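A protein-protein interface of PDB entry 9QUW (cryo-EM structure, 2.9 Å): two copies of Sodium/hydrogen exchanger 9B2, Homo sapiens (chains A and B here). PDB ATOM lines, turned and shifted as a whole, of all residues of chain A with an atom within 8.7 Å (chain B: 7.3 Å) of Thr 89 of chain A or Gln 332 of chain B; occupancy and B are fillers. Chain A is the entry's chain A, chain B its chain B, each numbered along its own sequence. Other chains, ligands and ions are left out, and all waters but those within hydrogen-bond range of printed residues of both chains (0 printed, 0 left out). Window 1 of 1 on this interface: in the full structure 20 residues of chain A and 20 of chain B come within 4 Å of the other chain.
The side-chain carboxylate of Asp 85 of chain A lies close to the backbone carbonyl oxygen of Phe 327 of chain B (2.6 Å).
The side-chain carboxylate (OD2) of Asp 85 of chain A lies within hydrogen-bond range of the side-chain hydroxyl (OG) of Ser 329 of chain B (3.2 Å).
The side-chain carboxylate (OD1) of Asp 85 of chain A sits at hydrogen-bond distance from the side-chain amide nitrogen (NE2) of Gln 332 of chain B (3.1 Å).
The backbone carbonyl oxygen of Asp 85 of chain A is in hydrogen-bond range of the side-chain hydroxyl of Thr 89 of chain A.
The backbone carbonyl oxygen (O) of Ile 88 of chain A sits at hydrogen-bond distance from the side-chain hydroxyl (OG1) of Thr 92 of chain A.
The side-chain hydroxyl (OG) of Ser 329 of chain B lies within hydrogen-bond range of the backbone carbonyl oxygen (O) of Phe 327 of chain B (3.5 Å).
The side-chain amide oxygen (OE1) of Gln 332 of chain B sits at hydrogen-bond distance from the side-chain amino group (NZ) of Lys 338 of chain B, at 2.9 Å.
The side-chain amino group (NZ) of Lys 338 of chain B is in salt-bridge range of the side-chain carboxylate (OD1) of Asp 333 of chain B (3.2 Å).
Ser 329 of chain B touches Pro 80 of chain A (OG to O, 3.9 Å).
Phe 327 of chain B touches Ile 88 of chain A.
OG1 of Thr 89 of chain A touches O of Phe 327 of chain B (3.8 Å).
Thr 89 of chain A touches Gln 332 of chain B.
Thr 92 of chain A touches Phe 323 of chain B.
Lys 338 of chain B touches Ile 93 of chain A (CG to CD1, 3.9 Å).
Leu 96 of chain A touches Leu 342 of chain B (CD2 to CD2, 3.5 Å).
Thr 89 of chain A touches two residues of chain B.
Of chain A, only Asp 85 and Thr 89 come within 4 Å of Gln 332 of chain B.
Printed residues of chain A within 4 Å of Leu 342 of chain B: Leu 96.
Printed residues of chain A within 4 Å of Phe 323 of chain B: Thr 92.
Ile 94 of chain A touches none of the printed residues of chain B.
The nearest residue of chain B that does not touch Thr 89 of chain A is Pro 328 of chain B (4.2 Å).
The nearest residue of chain A that does not touch Gln 332 of chain B is Arg 86 of chain A (4.4 Å).
The nearest printed residue of chain B that does not touch Ile 93 of chain A is Leu 342 of chain B (4.4 Å).
Hydrophobic or aromatic side chains of chain B that line the printed part of chain A: Phe 323, Phe 327 and Leu 342.
Along chain B the printed residues that touch a printed residue of chain A span positions 323 to 342.
Among the printed residues, no Asp or Glu carboxylate lies within 4 Å of a Lys or Arg side-chain nitrogen of the other chain.
No position is printed for both chains.
Of the 10 pairs that touch across the chains among the printed residues, none has its exchanged pair printed and touching as well.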
ATOM      1  N   PRO A  80      34.086   1.398 -29.344  1.00  0.00           N
ATOM      2  CA  PRO A  80      33.980   0.120 -28.629  1.00  0.00           C
ATOM      3  C   PRO A  80      35.025  -0.875 -29.104  1.00  0.00           C
ATOM      4  O   PRO A  80      35.363  -0.934 -30.289  1.00  0.00           O
ATOM      5  CB  PRO A  80      32.562  -0.357 -28.956  1.00  0.00           C
ATOM      6  CG  PRO A  80      31.830   0.851 -29.395  1.00  0.00           C
ATOM      7  CD  PRO A  80      32.831   1.761 -30.020  1.00  0.00           C
ATOM      8  N   HIS A  81      35.537  -1.664 -28.164  1.00  0.00           N
ATOM      9  CA  HIS A  81      36.536  -2.677 -28.467  1.00  0.00           C
ATOM     10  C   HIS A  81      36.834  -3.465 -27.201  1.00  0.00           C
ATOM     11  O   HIS A  81      36.682  -2.954 -26.089  1.00  0.00           O
ATOM     12  CB  HIS A  81      37.826  -2.045 -29.009  1.00  0.00           C
ATOM     13  CG  HIS A  81      38.594  -1.273 -27.982  1.00  0.00           C
ATOM     14  ND1 HIS A  81      38.080  -0.161 -27.351  1.00  0.00           N
ATOM     15  CD2 HIS A  81      39.836  -1.454 -27.476  1.00  0.00           C
ATOM     16  CE1 HIS A  81      38.974   0.311 -26.500  1.00  0.00           C
ATOM     17  NE2 HIS A  81      40.048  -0.455 -26.557  1.00  0.00           N
ATOM     18  N   GLY A  82      37.261  -4.708 -27.386  1.00  0.00           N
ATOM     19  CA  GLY A  82      37.740  -5.496 -26.273  1.00  0.00           C
ATOM     20  C   GLY A  82      36.630  -6.166 -25.485  1.00  0.00           C
ATOM     21  O   GLY A  82      35.518  -6.403 -25.965  1.00  0.00           O
ATOM     22  N   LEU A  83      36.960  -6.471 -24.229  1.00  0.00           N
ATOM     23  CA  LEU A  83      36.062  -7.252 -23.386  1.00  0.00           C
ATOM     24  C   LEU A  83      34.744  -6.522 -23.160  1.00  0.00           C
ATOM     25  O   LEU A  83      33.674  -7.143 -23.151  1.00  0.00           O
ATOM     26  CB  LEU A  83      36.753  -7.556 -22.056  1.00  0.00           C
ATOM     27  CG  LEU A  83      36.090  -8.521 -21.068  1.00  0.00           C
ATOM     28  CD1 LEU A  83      37.135  -9.308 -20.289  1.00  0.00           C
ATOM     29  CD2 LEU A  83      35.133  -7.796 -20.130  1.00  0.00           C
ATOM     30  N   LEU A  84      34.799  -5.202 -22.975  1.00  0.00           N
ATOM     31  CA  LEU A  84      33.586  -4.457 -22.659  1.00  0.00           C
ATOM     32  C   LEU A  84      32.570  -4.552 -23.789  1.00  0.00           C
ATOM     33  O   LEU A  84      31.373  -4.731 -23.542  1.00  0.00           O
ATOM     34  CB  LEU A  84      33.926  -2.997 -22.360  1.00  0.00           C
ATOM     35  CG  LEU A  84      34.509  -2.184 -23.515  1.00  0.00           C
ATOM     36  CD1 LEU A  84      33.433  -1.330 -24.159  1.00  0.00           C
ATOM     37  CD2 LEU A  84      35.658  -1.317 -23.027  1.00  0.00           C
ATOM     38  N   ASP A  85      33.019  -4.434 -25.037  1.00  0.00           N
ATOM     39  CA  ASP A  85      32.081  -4.544 -26.148  1.00  0.00           C
ATOM     40  C   ASP A  85      31.450  -5.926 -26.194  1.00  0.00           C
ATOM     41  O   ASP A  85      30.241  -6.060 -26.416  1.00  0.00           O
ATOM     42  CB  ASP A  85      32.781  -4.243 -27.470  1.00  0.00           C
ATOM     43  CG  ASP A  85      31.841  -4.324 -28.648  1.00  0.00           C
ATOM     44  OD1 ASP A  85      31.364  -5.436 -28.954  1.00  0.00           O
ATOM     45  OD2 ASP A  85      31.571  -3.276 -29.266  1.00  0.00           O
ATOM     46  N   ARG A  86      32.254  -6.970 -25.995  1.00  0.00           N
ATOM     47  CA  ARG A  86      31.718  -8.323 -26.043  1.00  0.00           C
ATOM     48  C   ARG A  86      30.681  -8.536 -24.951  1.00  0.00           C
ATOM     49  O   ARG A  86      29.618  -9.118 -25.198  1.00  0.00           O
ATOM     50  CB  ARG A  86      32.852  -9.335 -25.908  1.00  0.00           C
ATOM     51  CG  ARG A  86      32.382 -10.771 -25.807  1.00  0.00           C
ATOM     52  CD  ARG A  86      33.357 -11.729 -26.475  1.00  0.00           C
ATOM     53  NE  ARG A  86      34.569 -11.914 -25.684  1.00  0.00           N
ATOM     54  CZ  ARG A  86      34.619 -12.562 -24.529  1.00  0.00           C
ATOM     55  NH1 ARG A  86      33.537 -13.103 -23.990  1.00  0.00           N
ATOM     56  NH2 ARG A  86      35.785 -12.672 -23.897  1.00  0.00           N
ATOM     57  N   VAL A  87      30.964  -8.066 -23.736  1.00  0.00           N
ATOM     58  CA  VAL A  87      30.021  -8.280 -22.644  1.00  0.00           C
ATOM     59  C   VAL A  87      28.753  -7.470 -22.874  1.00  0.00           C
ATOM     60  O   VAL A  87      27.642  -7.945 -22.607  1.00  0.00           O
ATOM     61  CB  VAL A  87      30.678  -7.961 -21.288  1.00  0.00           C
ATOM     62  CG1 VAL A  87      30.666  -6.476 -21.001  1.00  0.00           C
ATOM     63  CG2 VAL A  87      29.981  -8.719 -20.177  1.00  0.00           C
ATOM     64  N   ILE A  88      28.887  -6.245 -23.389  1.00  0.00           N
ATOM     65  CA  ILE A  88      27.706  -5.439 -23.688  1.00  0.00           C
ATOM     66  C   ILE A  88      26.836  -6.151 -24.714  1.00  0.00           C
ATOM     67  O   ILE A  88      25.614  -6.259 -24.555  1.00  0.00           O
ATOM     68  CB  ILE A  88      28.120  -4.042 -24.181  1.00  0.00           C
ATOM     69  CG1 ILE A  88      28.876  -3.283 -23.088  1.00  0.00           C
ATOM     70  CG2 ILE A  88      26.901  -3.265 -24.634  1.00  0.00           C
ATOM     71  CD1 ILE A  88      27.998  -2.454 -22.178  1.00  0.00           C
ATOM     72  N   THR A  89      27.457  -6.658 -25.779  1.00  0.00           N
ATOM     73  CA  THR A  89      26.700  -7.341 -26.819  1.00  0.00           C
ATOM     74  C   THR A  89      26.010  -8.584 -26.277  1.00  0.00           C
ATOM     75  O   THR A  89      24.850  -8.850 -26.605  1.00  0.00           O
ATOM     76  CB  THR A  89      27.620  -7.717 -27.974  1.00  0.00           C
ATOM     77  OG1 THR A  89      28.370  -6.569 -28.383  1.00  0.00           O
ATOM     78  CG2 THR A  89      26.814  -8.242 -29.142  1.00  0.00           C
ATOM     79  N   ASN A  90      26.711  -9.370 -25.459  1.00  0.00           N
ATOM     80  CA  ASN A  90      26.118 -10.605 -24.960  1.00  0.00           C
ATOM     81  C   ASN A  90      24.956 -10.318 -24.018  1.00  0.00           C
ATOM     82  O   ASN A  90      23.903 -10.967 -24.102  1.00  0.00           O
ATOM     83  CB  ASN A  90      27.186 -11.446 -24.266  1.00  0.00           C
ATOM     84  CG  ASN A  90      28.011 -12.251 -25.244  1.00  0.00           C
ATOM     85  OD1 ASN A  90      28.097 -13.472 -25.142  1.00  0.00           O
ATOM     86  ND2 ASN A  90      28.626 -11.570 -26.201  1.00  0.00           N
ATOM     87  N   VAL A  91      25.123  -9.349 -23.115  1.00  0.00           N
ATOM     88  CA  VAL A  91      24.025  -8.971 -22.232  1.00  0.00           C
ATOM     89  C   VAL A  91      22.838  -8.494 -23.052  1.00  0.00           C
ATOM     90  O   VAL A  91      21.684  -8.848 -22.774  1.00  0.00           O
ATOM     91  CB  VAL A  91      24.494  -7.896 -21.236  1.00  0.00           C
ATOM     92  CG1 VAL A  91      23.309  -7.274 -20.531  1.00  0.00           C
ATOM     93  CG2 VAL A  91      25.463  -8.490 -20.235  1.00  0.00           C
ATOM     94  N   THR A  92      23.101  -7.679 -24.076  1.00  0.00           N
ATOM     95  CA  THR A  92      22.023  -7.185 -24.918  1.00  0.00           C
ATOM     96  C   THR A  92      21.296  -8.328 -25.605  1.00  0.00           C
ATOM     97  O   THR A  92      20.068  -8.338 -25.663  1.00  0.00           O
ATOM     98  CB  THR A  92      22.574  -6.214 -25.957  1.00  0.00           C
ATOM     99  OG1 THR A  92      22.979  -5.002 -25.309  1.00  0.00           O
ATOM    100  CG2 THR A  92      21.525  -5.903 -27.002  1.00  0.00           C
ATOM    101  N   ILE A  93      22.038  -9.299 -26.133  1.00  0.00           N
ATOM    102  CA  ILE A  93      21.400 -10.410 -26.832  1.00  0.00           C
ATOM    103  C   ILE A  93      20.532 -11.210 -25.874  1.00  0.00           C
ATOM    104  O   ILE A  93      19.414 -11.609 -26.214  1.00  0.00           O
ATOM    105  CB  ILE A  93      22.459 -11.294 -27.513  1.00  0.00           C
ATOM    106  CG1 ILE A  93      22.948 -10.636 -28.799  1.00  0.00           C
ATOM    107  CG2 ILE A  93      21.886 -12.659 -27.818  1.00  0.00           C
ATOM    108  CD1 ILE A  93      24.341 -11.038 -29.191  1.00  0.00           C
ATOM    109  N   ILE A  94      21.031 -11.465 -24.664  1.00  0.00           N
ATOM    110  CA  ILE A  94      20.252 -12.232 -23.694  1.00  0.00           C
ATOM    111  C   ILE A  94      18.950 -11.506 -23.370  1.00  0.00           C
ATOM    112  O   ILE A  94      17.845 -12.071 -23.469  1.00  0.00           O
ATOM    113  CB  ILE A  94      21.085 -12.468 -22.424  1.00  0.00           C
ATOM    114  CG1 ILE A  94      22.119 -13.565 -22.652  1.00  0.00           C
ATOM    115  CG2 ILE A  94      20.188 -12.825 -21.263  1.00  0.00           C
ATOM    116  CD1 ILE A  94      23.266 -13.510 -21.676  1.00  0.00           C
ATOM    117  N   VAL A  95      19.065 -10.234 -22.983  1.00  0.00           N
ATOM    118  CA  VAL A  95      17.887  -9.471 -22.594  1.00  0.00           C
ATOM    119  C   VAL A  95      16.923  -9.369 -23.760  1.00  0.00           C
ATOM    120  O   VAL A  95      15.703  -9.433 -23.586  1.00  0.00           O
ATOM    121  CB  VAL A  95      18.298  -8.082 -22.082  1.00  0.00           C
ATOM    122  CG1 VAL A  95      17.071  -7.248 -21.794  1.00  0.00           C
ATOM    123  CG2 VAL A  95      19.160  -8.206 -20.845  1.00  0.00           C
ATOM    124  N   LEU A  96      17.455  -9.218 -24.972  1.00  0.00           N
ATOM    125  CA  LEU A  96      16.609  -9.053 -26.143  1.00  0.00           C
ATOM    126  C   LEU A  96      15.865 -10.336 -26.473  1.00  0.00           C
ATOM    127  O   LEU A  96      14.706 -10.291 -26.889  1.00  0.00           O
ATOM    128  CB  LEU A  96      17.459  -8.608 -27.328  1.00  0.00           C
ATOM    129  CG  LEU A  96      16.820  -8.752 -28.703  1.00  0.00           C
ATOM    130  CD1 LEU A  96      15.573  -7.904 -28.777  1.00  0.00           C
ATOM    131  CD2 LEU A  96      17.814  -8.345 -29.762  1.00  0.00           C
ATOM    132  N   PHE B 323      22.780   2.332 -32.035  1.00  0.00           N
ATOM    133  CA  PHE B 323      23.346   1.333 -31.139  1.00  0.00           C
ATOM    134  C   PHE B 323      23.883   0.143 -31.918  1.00  0.00           C
ATOM    135  O   PHE B 323      25.088  -0.122 -31.912  1.00  0.00           O
ATOM    136  CB  PHE B 323      22.299   0.881 -30.126  1.00  0.00           C
ATOM    137  CG  PHE B 323      22.729  -0.300 -29.315  1.00  0.00           C
ATOM    138  CD1 PHE B 323      23.666  -0.161 -28.310  1.00  0.00           C
ATOM    139  CD2 PHE B 323      22.202  -1.552 -29.561  1.00  0.00           C
ATOM    140  CE1 PHE B 323      24.065  -1.246 -27.567  1.00  0.00           C
ATOM    141  CE2 PHE B 323      22.599  -2.638 -28.819  1.00  0.00           C
ATOM    142  CZ  PHE B 323      23.529  -2.484 -27.823  1.00  0.00           C
ATOM    143  N   TYR B 326      27.102   0.112 -34.118  1.00  0.00           N
ATOM    144  CA  TYR B 326      28.436   0.205 -33.545  1.00  0.00           C
ATOM    145  C   TYR B 326      28.832  -1.003 -32.722  1.00  0.00           C
ATOM    146  O   TYR B 326      30.005  -1.378 -32.727  1.00  0.00           O
ATOM    147  CB  TYR B 326      28.544   1.452 -32.662  1.00  0.00           C
ATOM    148  CG  TYR B 326      28.966   2.680 -33.414  1.00  0.00           C
ATOM    149  CD1 TYR B 326      30.177   2.716 -34.076  1.00  0.00           C
ATOM    150  CD2 TYR B 326      28.150   3.797 -33.473  1.00  0.00           C
ATOM    151  CE1 TYR B 326      30.572   3.827 -34.773  1.00  0.00           C
ATOM    152  CE2 TYR B 326      28.538   4.919 -34.165  1.00  0.00           C
ATOM    153  CZ  TYR B 326      29.750   4.928 -34.816  1.00  0.00           C
ATOM    154  OH  TYR B 326      30.151   6.040 -35.513  1.00  0.00           O
ATOM    155  N   PHE B 327      27.904  -1.612 -32.005  1.00  0.00           N
ATOM    156  CA  PHE B 327      28.370  -2.430 -30.900  1.00  0.00           C
ATOM    157  C   PHE B 327      28.775  -3.829 -31.328  1.00  0.00           C
ATOM    158  O   PHE B 327      29.885  -4.263 -30.997  1.00  0.00           O
ATOM    159  CB  PHE B 327      27.329  -2.474 -29.799  1.00  0.00           C
ATOM    160  CG  PHE B 327      27.689  -1.590 -28.669  1.00  0.00           C
ATOM    161  CD1 PHE B 327      28.614  -1.996 -27.735  1.00  0.00           C
ATOM    162  CD2 PHE B 327      27.174  -0.317 -28.591  1.00  0.00           C
ATOM    163  CE1 PHE B 327      28.979  -1.165 -26.714  1.00  0.00           C
ATOM    164  CE2 PHE B 327      27.534   0.517 -27.571  1.00  0.00           C
ATOM    165  CZ  PHE B 327      28.441   0.094 -26.629  1.00  0.00           C
ATOM    166  N   PRO B 328      27.964  -4.558 -32.060  1.00  0.00           N
ATOM    167  CA  PRO B 328      28.489  -5.803 -32.616  1.00  0.00           C
ATOM    168  C   PRO B 328      29.608  -5.424 -33.560  1.00  0.00           C
ATOM    169  O   PRO B 328      29.373  -4.956 -34.678  1.00  0.00           O
ATOM    170  CB  PRO B 328      27.282  -6.423 -33.328  1.00  0.00           C
ATOM    171  CG  PRO B 328      26.105  -5.804 -32.684  1.00  0.00           C
ATOM    172  CD  PRO B 328      26.506  -4.446 -32.206  1.00  0.00           C
ATOM    173  N   SER B 329      30.836  -5.611 -33.099  1.00  0.00           N
ATOM    174  CA  SER B 329      31.994  -4.997 -33.725  1.00  0.00           C
ATOM    175  C   SER B 329      32.478  -5.834 -34.895  1.00  0.00           C
ATOM    176  O   SER B 329      32.082  -6.985 -35.079  1.00  0.00           O
ATOM    177  CB  SER B 329      33.118  -4.820 -32.709  1.00  0.00           C
ATOM    178  OG  SER B 329      33.072  -3.534 -32.121  1.00  0.00           O
ATOM    179  N   ARG B 330      33.367  -5.242 -35.687  1.00  0.00           N
ATOM    180  CA  ARG B 330      33.865  -5.928 -36.868  1.00  0.00           C
ATOM    181  C   ARG B 330      34.793  -7.084 -36.521  1.00  0.00           C
ATOM    182  O   ARG B 330      35.171  -7.838 -37.423  1.00  0.00           O
ATOM    183  CB  ARG B 330      34.586  -4.944 -37.786  1.00  0.00           C
ATOM    184  CG  ARG B 330      34.041  -3.533 -37.725  1.00  0.00           C
ATOM    185  CD  ARG B 330      34.429  -2.734 -38.950  1.00  0.00           C
ATOM    186  NE  ARG B 330      33.398  -2.787 -39.980  1.00  0.00           N
ATOM    187  CZ  ARG B 330      32.297  -2.048 -39.982  1.00  0.00           C
ATOM    188  NH1 ARG B 330      32.037  -1.194 -39.007  1.00  0.00           N
ATOM    189  NH2 ARG B 330      31.435  -2.173 -40.985  1.00  0.00           N
ATOM    190  N   ASP B 331      35.159  -7.243 -35.250  1.00  0.00           N
ATOM    191  CA  ASP B 331      36.139  -8.240 -34.834  1.00  0.00           C
ATOM    192  C   ASP B 331      35.544  -9.311 -33.927  1.00  0.00           C
ATOM    193  O   ASP B 331      36.191  -9.716 -32.956  1.00  0.00           O
ATOM    194  CB  ASP B 331      37.311  -7.554 -34.136  1.00  0.00           C
ATOM    195  CG  ASP B 331      36.874  -6.709 -32.959  1.00  0.00           C
ATOM    196  OD1 ASP B 331      36.248  -7.256 -32.030  1.00  0.00           O
ATOM    197  OD2 ASP B 331      37.160  -5.494 -32.961  1.00  0.00           O
ATOM    198  N   GLN B 332      34.331  -9.774 -34.204  1.00  0.00           N
ATOM    199  CA  GLN B 332      33.716 -10.832 -33.418  1.00  0.00           C
ATOM    200  C   GLN B 332      33.508 -12.084 -34.264  1.00  0.00           C
ATOM    201  O   GLN B 332      33.531 -12.045 -35.496  1.00  0.00           O
ATOM    202  CB  GLN B 332      32.394 -10.357 -32.819  1.00  0.00           C
ATOM    203  CG  GLN B 332      32.583  -9.607 -31.513  1.00  0.00           C
ATOM    204  CD  GLN B 332      31.289  -9.373 -30.775  1.00  0.00           C
ATOM    205  OE1 GLN B 332      30.529 -10.304 -30.522  1.00  0.00           O
ATOM    206  NE2 GLN B 332      31.033  -8.122 -30.418  1.00  0.00           N
ATOM    207  N   ASP B 333      33.304 -13.208 -33.576  1.00  0.00           N
ATOM    208  CA  ASP B 333      33.416 -14.511 -34.226  1.00  0.00           C
ATOM    209  C   ASP B 333      32.251 -14.783 -35.173  1.00  0.00           C
ATOM    210  O   ASP B 333      32.444 -15.383 -36.238  1.00  0.00           O
ATOM    211  CB  ASP B 333      33.518 -15.620 -33.177  1.00  0.00           C
ATOM    212  CG  ASP B 333      32.491 -15.478 -32.065  1.00  0.00           C
ATOM    213  OD1 ASP B 333      31.306 -15.227 -32.367  1.00  0.00           O
ATOM    214  OD2 ASP B 333      32.871 -15.620 -30.885  1.00  0.00           O
ATOM    215  N   LYS B 334      31.044 -14.357 -34.813  1.00  0.00           N
ATOM    216  CA  LYS B 334      29.858 -14.705 -35.583  1.00  0.00           C
ATOM    217  C   LYS B 334      29.118 -13.441 -35.985  1.00  0.00           C
ATOM    218  O   LYS B 334      27.902 -13.340 -35.810  1.00  0.00           O
ATOM    219  CB  LYS B 334      28.946 -15.627 -34.782  1.00  0.00           C
ATOM    220  CG  LYS B 334      29.563 -16.975 -34.479  1.00  0.00           C
ATOM    221  CD  LYS B 334      28.525 -18.078 -34.528  1.00  0.00           C
ATOM    222  CE  LYS B 334      29.052 -19.367 -33.924  1.00  0.00           C
ATOM    223  NZ  LYS B 334      27.955 -20.184 -33.338  1.00  0.00           N
ATOM    224  N   LEU B 335      29.855 -12.478 -36.535  1.00  0.00           N
ATOM    225  CA  LEU B 335      29.318 -11.137 -36.728  1.00  0.00           C
ATOM    226  C   LEU B 335      27.990 -11.157 -37.473  1.00  0.00           C
ATOM    227  O   LEU B 335      27.025 -10.508 -37.057  1.00  0.00           O
ATOM    228  CB  LEU B 335      30.339 -10.288 -37.481  1.00  0.00           C
ATOM    229  CG  LEU B 335      30.048  -8.797 -37.506  1.00  0.00           C
ATOM    230  CD1 LEU B 335      29.822  -8.292 -36.102  1.00  0.00           C
ATOM    231  CD2 LEU B 335      31.192  -8.062 -38.164  1.00  0.00           C
ATOM    232  N   VAL B 336      27.921 -11.888 -38.582  1.00  0.00           N
ATOM    233  CA  VAL B 336      26.711 -11.865 -39.397  1.00  0.00           C
ATOM    234  C   VAL B 336      25.526 -12.393 -38.601  1.00  0.00           C
ATOM    235  O   VAL B 336      24.433 -11.815 -38.627  1.00  0.00           O
ATOM    236  CB  VAL B 336      26.922 -12.666 -40.694  1.00  0.00           C
ATOM    237  CG1 VAL B 336      25.587 -13.022 -41.317  1.00  0.00           C
ATOM    238  CG2 VAL B 336      27.769 -11.871 -41.663  1.00  0.00           C
ATOM    239  N   LYS B 338      25.069 -12.503 -35.330  1.00  0.00           N
ATOM    240  CA  LYS B 338      24.685 -11.588 -34.262  1.00  0.00           C
ATOM    241  C   LYS B 338      23.962 -10.370 -34.814  1.00  0.00           C
ATOM    242  O   LYS B 338      22.958  -9.929 -34.248  1.00  0.00           O
ATOM    243  CB  LYS B 338      25.918 -11.168 -33.471  1.00  0.00           C
ATOM    244  CG  LYS B 338      26.294 -12.161 -32.400  1.00  0.00           C
ATOM    245  CD  LYS B 338      27.469 -11.682 -31.573  1.00  0.00           C
ATOM    246  CE  LYS B 338      28.789 -12.202 -32.102  1.00  0.00           C
ATOM    247  NZ  LYS B 338      29.520 -12.941 -31.044  1.00  0.00           N
ATOM    248  N   LEU B 342      20.139  -9.351 -34.030  1.00  0.00           N
ATOM    249  CA  LEU B 342      19.845  -8.068 -33.411  1.00  0.00           C
ATOM    250  C   LEU B 342      18.794  -7.307 -34.204  1.00  0.00           C
ATOM    251  O   LEU B 342      17.792  -6.855 -33.643  1.00  0.00           O
ATOM    252  CB  LEU B 342      21.120  -7.242 -33.274  1.00  0.00           C
ATOM    253  CG  LEU B 342      21.896  -7.405 -31.964  1.00  0.00           C
ATOM    254  CD1 LEU B 342      23.031  -6.419 -31.921  1.00  0.00           C
ATOM    255  CD2 LEU B 342      21.004  -7.213 -30.756  1.00  0.00           C
